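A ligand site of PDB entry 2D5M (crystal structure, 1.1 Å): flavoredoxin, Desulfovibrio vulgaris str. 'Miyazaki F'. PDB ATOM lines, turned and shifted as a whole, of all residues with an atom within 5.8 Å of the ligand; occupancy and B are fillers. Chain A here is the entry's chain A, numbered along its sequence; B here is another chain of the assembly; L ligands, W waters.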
ATOM      1  N   LEU A  16     -24.296 -18.420 -13.180  1.00  0.00           N
ATOM      2  CA  LEU A  16     -22.951 -18.523 -12.635  1.00  0.00           C
ATOM      3  C   LEU A  16     -23.090 -18.518 -11.126  1.00  0.00           C
ATOM      4  O   LEU A  16     -22.987 -17.488 -10.456  1.00  0.00           O
ATOM      5  CB  LEU A  16     -22.014 -17.384 -13.128  1.00  0.00           C
ATOM      6  CG  LEU A  16     -20.549 -17.480 -12.660  1.00  0.00           C
ATOM      7  CD1 LEU A  16     -19.899 -18.732 -13.195  1.00  0.00           C
ATOM      8  CD2 LEU A  16     -19.777 -16.222 -13.043  1.00  0.00           C
ATOM      9  N   ASN A  29     -15.071 -23.079   1.171  1.00  0.00           N
ATOM     10  CA  ASN A  29     -14.788 -23.182  -0.246  1.00  0.00           C
ATOM     11  C   ASN A  29     -15.946 -22.632  -1.079  1.00  0.00           C
ATOM     12  O   ASN A  29     -17.068 -22.537  -0.601  1.00  0.00           O
ATOM     13  CB  ASN A  29     -14.572 -24.642  -0.633  1.00  0.00           C
ATOM     14  CG  ASN A  29     -13.869 -24.838  -1.964  1.00  0.00           C
ATOM     15  OD1 ASN A  29     -13.105 -23.955  -2.415  1.00  0.00           O
ATOM     16  ND2 ASN A  29     -14.081 -25.993  -2.578  1.00  0.00           N
ATOM     17  N   ILE A  30     -15.613 -22.271  -2.312  1.00  0.00           N
ATOM     18  CA  ILE A  30     -16.556 -21.908  -3.326  1.00  0.00           C
ATOM     19  C   ILE A  30     -16.055 -22.487  -4.641  1.00  0.00           C
ATOM     20  O   ILE A  30     -14.847 -22.470  -4.909  1.00  0.00           O
ATOM     21  CB  ILE A  30     -16.727 -20.376  -3.500  1.00  0.00           C
ATOM     22  CG1 ILE A  30     -15.407 -19.605  -3.301  1.00  0.00           C
ATOM     23  CG2 ILE A  30     -17.863 -19.873  -2.611  1.00  0.00           C
ATOM     24  CD1 ILE A  30     -15.438 -18.122  -3.631  1.00  0.00           C
ATOM     25  N   MET A  31     -17.003 -22.955  -5.472  1.00  0.00           N
ATOM     26  CA  MET A  31     -16.737 -23.361  -6.850  1.00  0.00           C
ATOM     27  C   MET A  31     -17.789 -22.757  -7.744  1.00  0.00           C
ATOM     28  O   MET A  31     -18.871 -22.402  -7.285  1.00  0.00           O
ATOM     29  CB  MET A  31     -16.633 -24.875  -7.026  1.00  0.00           C
ATOM     30  CG  MET A  31     -17.867 -25.627  -6.594  1.00  0.00           C
ATOM     31  SD  MET A  31     -19.198 -25.658  -7.804  1.00  0.00           S
ATOM     32  CE  MET A  31     -18.609 -26.851  -9.000  1.00  0.00           C
ATOM     33  N   ALA A  32     -17.502 -22.610  -9.034  1.00  0.00           N
ATOM     34  CA  ALA A  32     -18.477 -22.115  -9.990  1.00  0.00           C
ATOM     35  C   ALA A  32     -19.287 -23.267 -10.605  1.00  0.00           C
ATOM     36  O   ALA A  32     -18.710 -24.303 -11.002  1.00  0.00           O
ATOM     37  CB  ALA A  32     -17.762 -21.375 -11.107  1.00  0.00           C
ATOM     38  N   ALA A  33     -20.572 -23.055 -10.723  1.00  0.00           N
ATOM     39  CA  ALA A  33     -21.485 -24.023 -11.344  1.00  0.00           C
ATOM     40  C   ALA A  33     -22.457 -23.289 -12.272  1.00  0.00           C
ATOM     41  O   ALA A  33     -23.161 -22.397 -11.828  1.00  0.00           O
ATOM     42  CB  ALA A  33     -22.264 -24.814 -10.333  1.00  0.00           C
ATOM     43  N   ALA A  34     -22.493 -23.713 -13.526  1.00  0.00           N
ATOM     44  CA  ALA A  34     -23.481 -23.260 -14.484  1.00  0.00           C
ATOM     45  C   ALA A  34     -24.495 -24.327 -14.869  1.00  0.00           C
ATOM     46  O   ALA A  34     -25.546 -24.000 -15.445  1.00  0.00           O
ATOM     47  CB  ALA A  34     -22.825 -22.726 -15.747  1.00  0.00           C
ATOM     48  N   TRP A  35     -24.202 -25.619 -14.607  1.00  0.00           N
ATOM     49  CA  TRP A  35     -25.111 -26.717 -14.932  1.00  0.00           C
ATOM     50  C   TRP A  35     -26.051 -26.854 -13.735  1.00  0.00           C
ATOM     51  O   TRP A  35     -25.916 -27.708 -12.868  1.00  0.00           O
ATOM     52  CB  TRP A  35     -24.368 -28.002 -15.197  1.00  0.00           C
ATOM     53  CG  TRP A  35     -23.649 -28.172 -16.508  1.00  0.00           C
ATOM     54  CD1 TRP A  35     -23.137 -29.364 -16.893  1.00  0.00           C
ATOM     55  CD2 TRP A  35     -23.350 -27.263 -17.576  1.00  0.00           C
ATOM     56  NE1 TRP A  35     -22.547 -29.267 -18.117  1.00  0.00           N
ATOM     57  CE2 TRP A  35     -22.655 -27.985 -18.567  1.00  0.00           C
ATOM     58  CE3 TRP A  35     -23.609 -25.909 -17.836  1.00  0.00           C
ATOM     59  CZ2 TRP A  35     -22.211 -27.418 -19.753  1.00  0.00           C
ATOM     60  CZ3 TRP A  35     -23.158 -25.325 -19.006  1.00  0.00           C
ATOM     61  CH2 TRP A  35     -22.462 -26.093 -19.974  1.00  0.00           C
ATOM     62  N   ALA A  36     -27.005 -25.933 -13.655  1.00  0.00           N
ATOM     63  CA  ALA A  36     -27.787 -25.699 -12.470  1.00  0.00           C
ATOM     64  C   ALA A  36     -29.025 -24.902 -12.807  1.00  0.00           C
ATOM     65  O   ALA A  36     -29.056 -24.176 -13.795  1.00  0.00           O
ATOM     66  CB  ALA A  36     -26.967 -24.930 -11.415  1.00  0.00           C
ATOM     67  N   VAL A  48     -28.024 -28.836  -8.856  1.00  0.00           N
ATOM     68  CA  VAL A  48     -26.674 -28.483  -9.320  1.00  0.00           C
ATOM     69  C   VAL A  48     -25.965 -29.773  -9.714  1.00  0.00           C
ATOM     70  O   VAL A  48     -25.937 -30.715  -8.921  1.00  0.00           O
ATOM     71  CB  VAL A  48     -25.892 -27.728  -8.248  1.00  0.00           C
ATOM     72  CG1 VAL A  48     -24.694 -27.138  -8.992  1.00  0.00           C
ATOM     73  CG2 VAL A  48     -26.661 -26.662  -7.501  1.00  0.00           C
ATOM     74  N   SER A  49     -25.426 -29.807 -10.895  1.00  0.00           N
ATOM     75  CA  SER A  49     -24.666 -30.969 -11.365  1.00  0.00           C
ATOM     76  C   SER A  49     -23.207 -30.757 -11.062  1.00  0.00           C
ATOM     77  O   SER A  49     -22.587 -29.986 -11.775  1.00  0.00           O
ATOM     78  CB  SER A  49     -24.894 -31.133 -12.865  1.00  0.00           C
ATOM     79  OG  SER A  49     -26.215 -31.428 -13.151  1.00  0.00           O
ATOM     80  N   LEU A  50     -22.666 -31.420 -10.056  1.00  0.00           N
ATOM     81  CA  LEU A  50     -21.293 -31.285  -9.625  1.00  0.00           C
ATOM     82  C   LEU A  50     -20.560 -32.591  -9.833  1.00  0.00           C
ATOM     83  O   LEU A  50     -21.002 -33.642  -9.397  1.00  0.00           O
ATOM     84  CB  LEU A  50     -21.217 -30.886  -8.138  1.00  0.00           C
ATOM     85  CG  LEU A  50     -21.979 -29.624  -7.713  1.00  0.00           C
ATOM     86  CD1 LEU A  50     -21.742 -29.234  -6.272  1.00  0.00           C
ATOM     87  CD2 LEU A  50     -21.629 -28.461  -8.670  1.00  0.00           C
ATOM     88  N   ARG A  51     -19.417 -32.500 -10.482  1.00  0.00           N
ATOM     89  CA  ARG A  51     -18.603 -33.660 -10.752  1.00  0.00           C
ATOM     90  C   ARG A  51     -17.940 -34.195  -9.510  1.00  0.00           C
ATOM     91  O   ARG A  51     -17.529 -33.494  -8.602  1.00  0.00           O
ATOM     92  CB  ARG A  51     -17.512 -33.318 -11.795  1.00  0.00           C
ATOM     93  CG  ARG A  51     -18.065 -33.053 -13.163  1.00  0.00           C
ATOM     94  CD  ARG A  51     -17.062 -32.461 -14.184  1.00  0.00           C
ATOM     95  NE  ARG A  51     -16.745 -31.163 -13.615  1.00  0.00           N
ATOM     96  CZ  ARG A  51     -15.642 -30.827 -12.931  1.00  0.00           C
ATOM     97  NH1 ARG A  51     -14.593 -31.611 -12.823  1.00  0.00           N
ATOM     98  NH2 ARG A  51     -15.631 -29.623 -12.373  1.00  0.00           N
ATOM     99  N   ALA A  53     -15.008 -35.286  -9.130  1.00  0.00           N
ATOM    100  CA  ALA A  53     -13.643 -34.845  -8.961  1.00  0.00           C
ATOM    101  C   ALA A  53     -13.555 -33.554  -8.167  1.00  0.00           C
ATOM    102  O   ALA A  53     -12.473 -33.199  -7.679  1.00  0.00           O
ATOM    103  CB  ALA A  53     -12.955 -34.650 -10.315  1.00  0.00           C
ATOM    104  N   THR A  54     -14.640 -32.782  -8.064  1.00  0.00           N
ATOM    105  CA  THR A  54     -14.545 -31.513  -7.359  1.00  0.00           C
ATOM    106  C   THR A  54     -14.425 -31.741  -5.845  1.00  0.00           C
ATOM    107  O   THR A  54     -15.013 -32.673  -5.294  1.00  0.00           O
ATOM    108  CB  THR A  54     -15.719 -30.583  -7.649  1.00  0.00           C
ATOM    109  OG1 THR A  54     -16.911 -31.134  -7.152  1.00  0.00           O
ATOM    110  CG2 THR A  54     -15.874 -30.304  -9.110  1.00  0.00           C
ATOM    111  N   TYR A  55     -13.658 -30.870  -5.205  1.00  0.00           N
ATOM    112  CA  TYR A  55     -13.553 -30.970  -3.724  1.00  0.00           C
ATOM    113  C   TYR A  55     -14.932 -30.692  -3.099  1.00  0.00           C
ATOM    114  O   TYR A  55     -15.324 -31.276  -2.081  1.00  0.00           O
ATOM    115  CB  TYR A  55     -12.476 -30.020  -3.257  1.00  0.00           C
ATOM    116  CG  TYR A  55     -12.019 -30.205  -1.839  1.00  0.00           C
ATOM    117  CD1 TYR A  55     -11.444 -31.425  -1.460  1.00  0.00           C
ATOM    118  CD2 TYR A  55     -12.129 -29.237  -0.865  1.00  0.00           C
ATOM    119  CE1 TYR A  55     -10.988 -31.683  -0.186  1.00  0.00           C
ATOM    120  CE2 TYR A  55     -11.667 -29.448   0.431  1.00  0.00           C
ATOM    121  CZ  TYR A  55     -11.118 -30.666   0.792  1.00  0.00           C
ATOM    122  OH  TYR A  55     -10.645 -30.960   2.043  1.00  0.00           O
ATOM    123  N   THR A  56     -15.682 -29.765  -3.702  1.00  0.00           N
ATOM    124  CA  THR A  56     -17.010 -29.426  -3.230  1.00  0.00           C
ATOM    125  C   THR A  56     -17.939 -30.611  -3.172  1.00  0.00           C
ATOM    126  O   THR A  56     -18.734 -30.725  -2.233  1.00  0.00           O
ATOM    127  CB  THR A  56     -17.582 -28.339  -4.170  1.00  0.00           C
ATOM    128  OG1 THR A  56     -16.762 -27.170  -4.052  1.00  0.00           O
ATOM    129  CG2 THR A  56     -18.982 -27.954  -3.830  1.00  0.00           C
ATOM    130  N   TYR A  57     -17.913 -31.524  -4.066  1.00  0.00           N
ATOM    131  CA  TYR A  57     -18.681 -32.735  -4.122  1.00  0.00           C
ATOM    132  C   TYR A  57     -18.518 -33.466  -2.793  1.00  0.00           C
ATOM    133  O   TYR A  57     -19.495 -33.899  -2.159  1.00  0.00           O
ATOM    134  CB  TYR A  57     -18.300 -33.600  -5.340  1.00  0.00           C
ATOM    135  CG  TYR A  57     -19.074 -34.901  -5.459  1.00  0.00           C
ATOM    136  CD1 TYR A  57     -20.018 -35.068  -6.421  1.00  0.00           C
ATOM    137  CD2 TYR A  57     -18.825 -36.019  -4.694  1.00  0.00           C
ATOM    138  CE1 TYR A  57     -20.730 -36.247  -6.581  1.00  0.00           C
ATOM    139  CE2 TYR A  57     -19.500 -37.177  -4.806  1.00  0.00           C
ATOM    140  CZ  TYR A  57     -20.464 -37.294  -5.764  1.00  0.00           C
ATOM    141  OH  TYR A  57     -21.154 -38.498  -5.900  1.00  0.00           O
ATOM    142  N   ALA A  79     -15.270 -15.061  -9.436  1.00  0.00           N
ATOM    143  CA  ALA A  79     -16.105 -16.204  -9.735  1.00  0.00           C
ATOM    144  C   ALA A  79     -15.400 -17.147 -10.693  1.00  0.00           C
ATOM    145  O   ALA A  79     -15.400 -18.374 -10.524  1.00  0.00           O
ATOM    146  CB  ALA A  79     -17.448 -15.748 -10.262  1.00  0.00           C
ATOM    147  N   ASP A  80     -14.780 -16.556 -11.732  1.00  0.00           N
ATOM    148  CA  ASP A  80     -14.027 -17.357 -12.687  1.00  0.00           C
ATOM    149  C   ASP A  80     -12.893 -18.110 -12.011  1.00  0.00           C
ATOM    150  O   ASP A  80     -12.683 -19.310 -12.271  1.00  0.00           O
ATOM    151  CB  ASP A  80     -13.551 -16.464 -13.819  1.00  0.00           C
ATOM    152  CG  ASP A  80     -13.108 -17.233 -15.051  1.00  0.00           C
ATOM    153  OD1 ASP A  80     -13.937 -18.061 -15.553  1.00  0.00           O
ATOM    154  OD2 ASP A  80     -11.971 -17.014 -15.526  1.00  0.00           O
ATOM    155  N   TYR A  81     -12.149 -17.431 -11.128  1.00  0.00           N
ATOM    156  CA  TYR A  81     -11.083 -18.055 -10.383  1.00  0.00           C
ATOM    157  C   TYR A  81     -11.589 -19.303  -9.676  1.00  0.00           C
ATOM    158  O   TYR A  81     -10.955 -20.353  -9.693  1.00  0.00           O
ATOM    159  CB  TYR A  81     -10.495 -17.053  -9.389  1.00  0.00           C
ATOM    160  CG  TYR A  81      -9.319 -17.523  -8.598  1.00  0.00           C
ATOM    161  CD1 TYR A  81      -8.009 -17.129  -8.960  1.00  0.00           C
ATOM    162  CD2 TYR A  81      -9.444 -18.321  -7.462  1.00  0.00           C
ATOM    163  CE1 TYR A  81      -6.924 -17.535  -8.239  1.00  0.00           C
ATOM    164  CE2 TYR A  81      -8.346 -18.754  -6.754  1.00  0.00           C
ATOM    165  CZ  TYR A  81      -7.075 -18.343  -7.156  1.00  0.00           C
ATOM    166  OH  TYR A  81      -5.971 -18.760  -6.432  1.00  0.00           O
ATOM    167  N   ALA A  82     -12.719 -19.165  -8.998  1.00  0.00           N
ATOM    168  CA  ALA A  82     -13.313 -20.274  -8.227  1.00  0.00           C
ATOM    169  C   ALA A  82     -13.692 -21.438  -9.111  1.00  0.00           C
ATOM    170  O   ALA A  82     -13.829 -22.577  -8.625  1.00  0.00           O
ATOM    171  CB  ALA A  82     -14.532 -19.772  -7.440  1.00  0.00           C
ATOM    172  N   GLY A  83     -13.921 -21.164 -10.404  1.00  0.00           N
ATOM    173  CA  GLY A  83     -14.196 -22.187 -11.429  1.00  0.00           C
ATOM    174  C   GLY A  83     -13.001 -22.734 -12.147  1.00  0.00           C
ATOM    175  O   GLY A  83     -13.191 -23.603 -13.016  1.00  0.00           O
ATOM    176  N   ILE A  84     -11.803 -22.234 -11.870  1.00  0.00           N
ATOM    177  CA  ILE A  84     -10.572 -22.735 -12.460  1.00  0.00           C
ATOM    178  C   ILE A  84      -9.769 -23.563 -11.477  1.00  0.00           C
ATOM    179  O   ILE A  84      -9.245 -24.613 -11.809  1.00  0.00           O
ATOM    180  CB  ILE A  84      -9.734 -21.558 -12.998  1.00  0.00           C
ATOM    181  CG1 ILE A  84     -10.436 -20.794 -14.111  1.00  0.00           C
ATOM    182  CG2 ILE A  84      -8.327 -22.060 -13.414  1.00  0.00           C
ATOM    183  CD1 ILE A  84      -9.801 -19.459 -14.480  1.00  0.00           C
ATOM    184  N   TYR A  85      -9.645 -23.106 -10.231  1.00  0.00           N
ATOM    185  CA  TYR A  85      -8.772 -23.672  -9.226  1.00  0.00           C
ATOM    186  C   TYR A  85      -9.582 -24.454  -8.213  1.00  0.00           C
ATOM    187  O   TYR A  85     -10.726 -24.159  -7.969  1.00  0.00           O
ATOM    188  CB  TYR A  85      -7.907 -22.590  -8.565  1.00  0.00           C
ATOM    189  CG  TYR A  85      -7.132 -21.828  -9.637  1.00  0.00           C
ATOM    190  CD1 TYR A  85      -6.087 -22.454 -10.323  1.00  0.00           C
ATOM    191  CD2 TYR A  85      -7.448 -20.544  -9.961  1.00  0.00           C
ATOM    192  CE1 TYR A  85      -5.367 -21.792 -11.304  1.00  0.00           C
ATOM    193  CE2 TYR A  85      -6.763 -19.858 -10.960  1.00  0.00           C
ATOM    194  CZ  TYR A  85      -5.704 -20.499 -11.623  1.00  0.00           C
ATOM    195  OH  TYR A  85      -5.016 -19.821 -12.633  1.00  0.00           O
ATOM    196  N   SER A  86      -8.951 -25.483  -7.617  1.00  0.00           N
ATOM    197  CA  SER A  86      -9.588 -26.288  -6.627  1.00  0.00           C
ATOM    198  C   SER A  86      -9.271 -25.865  -5.196  1.00  0.00           C
ATOM    199  O   SER A  86      -8.138 -25.463  -4.896  1.00  0.00           O
ATOM    200  CB  SER A  86      -9.176 -27.774  -6.772  1.00  0.00           C
ATOM    201  OG  SER A  86      -9.844 -28.560  -5.778  1.00  0.00           O
ATOM    202  N   GLY A  87     -10.224 -26.054  -4.302  1.00  0.00           N
ATOM    203  CA  GLY A  87     -10.045 -25.811  -2.899  1.00  0.00           C
ATOM    204  C   GLY A  87      -9.483 -26.962  -2.103  1.00  0.00           C
ATOM    205  O   GLY A  87      -9.323 -26.834  -0.890  1.00  0.00           O
ATOM    206  N   GLU A  88      -9.142 -28.067  -2.730  1.00  0.00           N
ATOM    207  CA  GLU A  88      -8.618 -29.219  -1.979  1.00  0.00           C
ATOM    208  C   GLU A  88      -7.435 -28.808  -1.104  1.00  0.00           C
ATOM    209  O   GLU A  88      -7.366 -29.225   0.076  1.00  0.00           O
ATOM    210  CB  GLU A  88      -8.259 -30.340  -2.935  1.00  0.00           C
ATOM    211  CG  GLU A  88      -7.769 -31.587  -2.225  1.00  0.00           C
ATOM    212  CD  GLU A  88      -7.232 -32.674  -3.138  1.00  0.00           C
ATOM    213  OE1 GLU A  88      -7.203 -32.550  -4.377  1.00  0.00           O
ATOM    214  OE2 GLU A  88      -6.807 -33.683  -2.551  1.00  0.00           O
ATOM    215  N   LYS A  92      -9.654 -20.491  -1.116  1.00  0.00           N
ATOM    216  CA  LYS A  92      -9.953 -19.516  -2.140  1.00  0.00           C
ATOM    217  C   LYS A  92     -10.462 -18.206  -1.580  1.00  0.00           C
ATOM    218  O   LYS A  92     -10.316 -17.162  -2.210  1.00  0.00           O
ATOM    219  CB  LYS A  92     -10.971 -20.066  -3.129  1.00  0.00           C
ATOM    220  CG  LYS A  92     -10.574 -21.277  -3.887  1.00  0.00           C
ATOM    221  CD  LYS A  92     -11.663 -21.717  -4.866  1.00  0.00           C
ATOM    222  CE  LYS A  92     -11.578 -23.188  -5.104  1.00  0.00           C
ATOM    223  NZ  LYS A  92     -12.652 -23.727  -5.948  1.00  0.00           N
ATOM    224  N   PHE A 164     -23.580 -16.822 -17.796  1.00  0.00           N
ATOM    225  CA  PHE A 164     -22.584 -17.575 -18.513  1.00  0.00           C
ATOM    226  C   PHE A 164     -23.096 -18.001 -19.890  1.00  0.00           C
ATOM    227  O   PHE A 164     -24.209 -18.502 -20.001  1.00  0.00           O
ATOM    228  CB  PHE A 164     -22.110 -18.778 -17.714  1.00  0.00           C
ATOM    229  CG  PHE A 164     -21.148 -19.725 -18.385  1.00  0.00           C
ATOM    230  CD1 PHE A 164     -19.901 -19.243 -18.835  1.00  0.00           C
ATOM    231  CD2 PHE A 164     -21.426 -21.035 -18.580  1.00  0.00           C
ATOM    232  CE1 PHE A 164     -18.991 -20.090 -19.396  1.00  0.00           C
ATOM    233  CE2 PHE A 164     -20.509 -21.900 -19.100  1.00  0.00           C
ATOM    234  CZ  PHE A 164     -19.277 -21.441 -19.538  1.00  0.00           C
ATOM    235  N   TYR A 171     -18.840 -14.279 -20.205  1.00  0.00           N
ATOM    236  CA  TYR A 171     -19.734 -13.768 -19.182  1.00  0.00           C
ATOM    237  C   TYR A 171     -20.383 -12.471 -19.645  1.00  0.00           C
ATOM    238  O   TYR A 171     -19.683 -11.619 -20.197  1.00  0.00           O
ATOM    239  CB  TYR A 171     -18.943 -13.510 -17.920  1.00  0.00           C
ATOM    240  CG  TYR A 171     -18.296 -14.713 -17.267  1.00  0.00           C
ATOM    241  CD1 TYR A 171     -16.959 -14.736 -17.019  1.00  0.00           C
ATOM    242  CD2 TYR A 171     -19.046 -15.815 -16.899  1.00  0.00           C
ATOM    243  CE1 TYR A 171     -16.330 -15.826 -16.425  1.00  0.00           C
ATOM    244  CE2 TYR A 171     -18.439 -16.901 -16.268  1.00  0.00           C
ATOM    245  CZ  TYR A 171     -17.095 -16.892 -16.033  1.00  0.00           C
ATOM    246  OH  TYR A 171     -16.571 -17.978 -15.408  1.00  0.00           O
ATOM    247  N   ALA B 181     -14.539 -16.441 -19.844  1.00  0.00           N
ATOM    248  CA  ALA B 181     -14.520 -17.510 -18.876  1.00  0.00           C
ATOM    249  C   ALA B 181     -13.280 -18.368 -19.053  1.00  0.00           C
ATOM    250  O   ALA B 181     -12.715 -18.473 -20.133  1.00  0.00           O
ATOM    251  CB  ALA B 181     -15.813 -18.352 -18.974  1.00  0.00           C
ATOM    252  N   PHE B 182     -12.883 -19.000 -17.949  1.00  0.00           N
ATOM    253  CA  PHE B 182     -11.664 -19.798 -17.917  1.00  0.00           C
ATOM    254  C   PHE B 182     -10.484 -18.981 -18.364  1.00  0.00           C
ATOM    255  O   PHE B 182      -9.623 -19.406 -19.102  1.00  0.00           O
ATOM    256  CB  PHE B 182     -11.777 -21.121 -18.704  1.00  0.00           C
ATOM    257  CG  PHE B 182     -13.002 -21.931 -18.345  1.00  0.00           C
ATOM    258  CD1 PHE B 182     -14.147 -21.817 -19.091  1.00  0.00           C
ATOM    259  CD2 PHE B 182     -13.064 -22.791 -17.255  1.00  0.00           C
ATOM    260  CE1 PHE B 182     -15.281 -22.513 -18.734  1.00  0.00           C
ATOM    261  CE2 PHE B 182     -14.211 -23.488 -16.891  1.00  0.00           C
ATOM    262  CZ  PHE B 182     -15.337 -23.349 -17.657  1.00  0.00           C
HETATM  263  N1  LIG L   1     -18.018 -27.873 -12.442  1.00  0.00           N
HETATM  264  C1  LIG L   1     -19.063 -28.713 -12.127  1.00  0.00           C
HETATM  265  O1  LIG L   1     -18.852 -29.813 -11.607  1.00  0.00           O
HETATM  266  N2  LIG L   1     -20.353 -28.300 -12.431  1.00  0.00           N
HETATM  267  C2  LIG L   1     -20.692 -27.128 -13.064  1.00  0.00           C
HETATM  268  O2  LIG L   1     -21.884 -26.851 -13.300  1.00  0.00           O
HETATM  269  C3  LIG L   1     -19.607 -26.286 -13.440  1.00  0.00           C
HETATM  270  N3  LIG L   1     -19.858 -25.144 -14.126  1.00  0.00           N
HETATM  271  C4  LIG L   1     -18.793 -24.310 -14.307  1.00  0.00           C
HETATM  272  C5  LIG L   1     -19.029 -23.086 -14.992  1.00  0.00           C
HETATM  273  C6  LIG L   1     -18.042 -22.134 -15.207  1.00  0.00           C
HETATM  274  C7  LIG L   1     -18.292 -20.863 -15.973  1.00  0.00           C
HETATM  275  C8  LIG L   1     -16.739 -22.412 -14.657  1.00  0.00           C
HETATM  276  C9  LIG L   1     -15.648 -21.354 -14.784  1.00  0.00           C
HETATM  277  C10 LIG L   1     -16.475 -23.629 -14.058  1.00  0.00           C
HETATM  278  C11 LIG L   1     -17.466 -24.576 -13.865  1.00  0.00           C
HETATM  279  N4  LIG L   1     -17.252 -25.842 -13.281  1.00  0.00           N
HETATM  280  C12 LIG L   1     -18.303 -26.673 -13.009  1.00  0.00           C
HETATM  281  C13 LIG L   1     -15.869 -26.244 -12.869  1.00  0.00           C
HETATM  282  C14 LIG L   1     -15.631 -26.100 -11.371  1.00  0.00           C
HETATM  283  O3  LIG L   1     -16.051 -24.829 -10.864  1.00  0.00           O
HETATM  284  C15 LIG L   1     -14.136 -26.257 -11.109  1.00  0.00           C
HETATM  285  O4  LIG L   1     -13.804 -27.645 -11.389  1.00  0.00           O
HETATM  286  C16 LIG L   1     -13.700 -25.879  -9.702  1.00  0.00           C
HETATM  287  O5  LIG L   1     -12.250 -25.750  -9.750  1.00  0.00           O
HETATM  288  C17 LIG L   1     -14.057 -26.885  -8.662  1.00  0.00           C
HETATM  289  O6  LIG L   1     -13.557 -26.391  -7.371  1.00  0.00           O
HETATM  290  P1  LIG L   1     -13.441 -27.367  -6.096  1.00  0.00           P
HETATM  291  O7  LIG L   1     -12.521 -28.535  -6.472  1.00  0.00           O
HETATM  292  O8  LIG L   1     -14.803 -27.882  -5.690  1.00  0.00           O
HETATM  293  O9  LIG L   1     -12.808 -26.428  -5.089  1.00  0.00           O
HETATM  294  O   HOH W   1     -10.231 -27.427 -10.633  1.00  0.00           O
HETATM  295  O   HOH W   2     -11.556 -27.630 -12.925  1.00  0.00           O
HETATM  296  O   HOH W   3     -11.564 -29.411  -8.887  1.00  0.00           O
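N of Thr 56 is in hydrogen-bond range of O8 of the ligand, at 2.9 Å. OG1 of Thr 56 sits at hydrogen-bond distance from O8 of the ligand (2.7 Å). N of Ala 32 lies within hydrogen-bond range of O3 of the ligand (3.2 Å). An oxygen (O3) of the ligand sits at hydrogen-bond distance from the backbone carbonyl oxygen (O) of Ala 32 (2.7 Å). N of Gly 87 lies within hydrogen-bond range of O9 of the ligand (2.7 Å). An oxygen (O7) of the ligand sits at hydrogen-bond distance from the side-chain hydroxyl (OG) of Ser 86. An oxygen (O5) of the ligand lies within hydrogen-bond range of the backbone carbonyl oxygen of Tyr 85, at 2.8 Å. An oxygen (O9) of the ligand lies within salt-bridge range of the side-chain amino group (NZ) of Lys 92 (2.8 Å). The side-chain amide nitrogen (ND2) of Asn 29 sits at hydrogen-bond distance from an oxygen (O9) of the ligand, 2.8 Å away. O1 of the ligand sits at hydrogen-bond distance from N of Arg 51, at 3.0 Å. An oxygen (O4) of the ligand sits at hydrogen-bond distance from the guanidinium group (NH2) of Arg 51 (2.9 Å). O of Ser 49 sits at hydrogen-bond distance from N2 of the ligand (2.9 Å). N of Tyr 55 sits at hydrogen-bond distance from O7 of the ligand (2.9 Å). N of Trp 35 is in hydrogen-bond range of O2 of the ligand (2.9 Å). N of Ala 34 lies within hydrogen-bond range of N3 of the ligand, 3.1 Å away.
The backbone NH (N) of Glu 88 is in hydrogen-bond range of the side-chain hydroxyl (OG) of Ser 86 (3.2 Å). The side-chain amino group of Lys 92 sits at hydrogen-bond distance from the backbone carbonyl oxygen of Tyr 85. The backbone carbonyl oxygen (O) of Ala 82 lies within hydrogen-bond range of the side-chain amino group (NZ) of Lys 92 (3.1 Å). The side-chain amino group of Lys 92 is in hydrogen-bond range of the backbone carbonyl oxygen of Ile 30 (2.7 Å). O of Arg 51 is in hydrogen-bond range of OG1 of Thr 54 (2.8 Å). O of Trp 35 sits at hydrogen-bond distance from N of Ser 49. The backbone NH (N) of Phe 182 of chain B is in hydrogen-bond range of the side-chain carboxylate (OD1) of Asp 80 (2.8 Å). The backbone NH of Tyr 57 sits at hydrogen-bond distance from the side-chain hydroxyl of Thr 54, at 3.3 Å.
Merely in contact with the ligand: Gly 83 (3.3 Å), Phe 182 of chain B (3.3 Å), Tyr 171 (3.4 Å), Ala 33 (3.4 Å), Met 31 (3.4 Å), Thr 54 (3.5 Å), Leu 50 (3.5 Å), Ala 82 (3.5 Å), Phe 164 (3.6 Å), Ile 84 (3.7 Å), Asp 80 (3.8 Å) and Leu 16 (3.9 Å).
Water W1 lies within hydrogen-bond range of O5 of the ligand (2.8 Å) and O of Ile 84 (3.2 Å).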
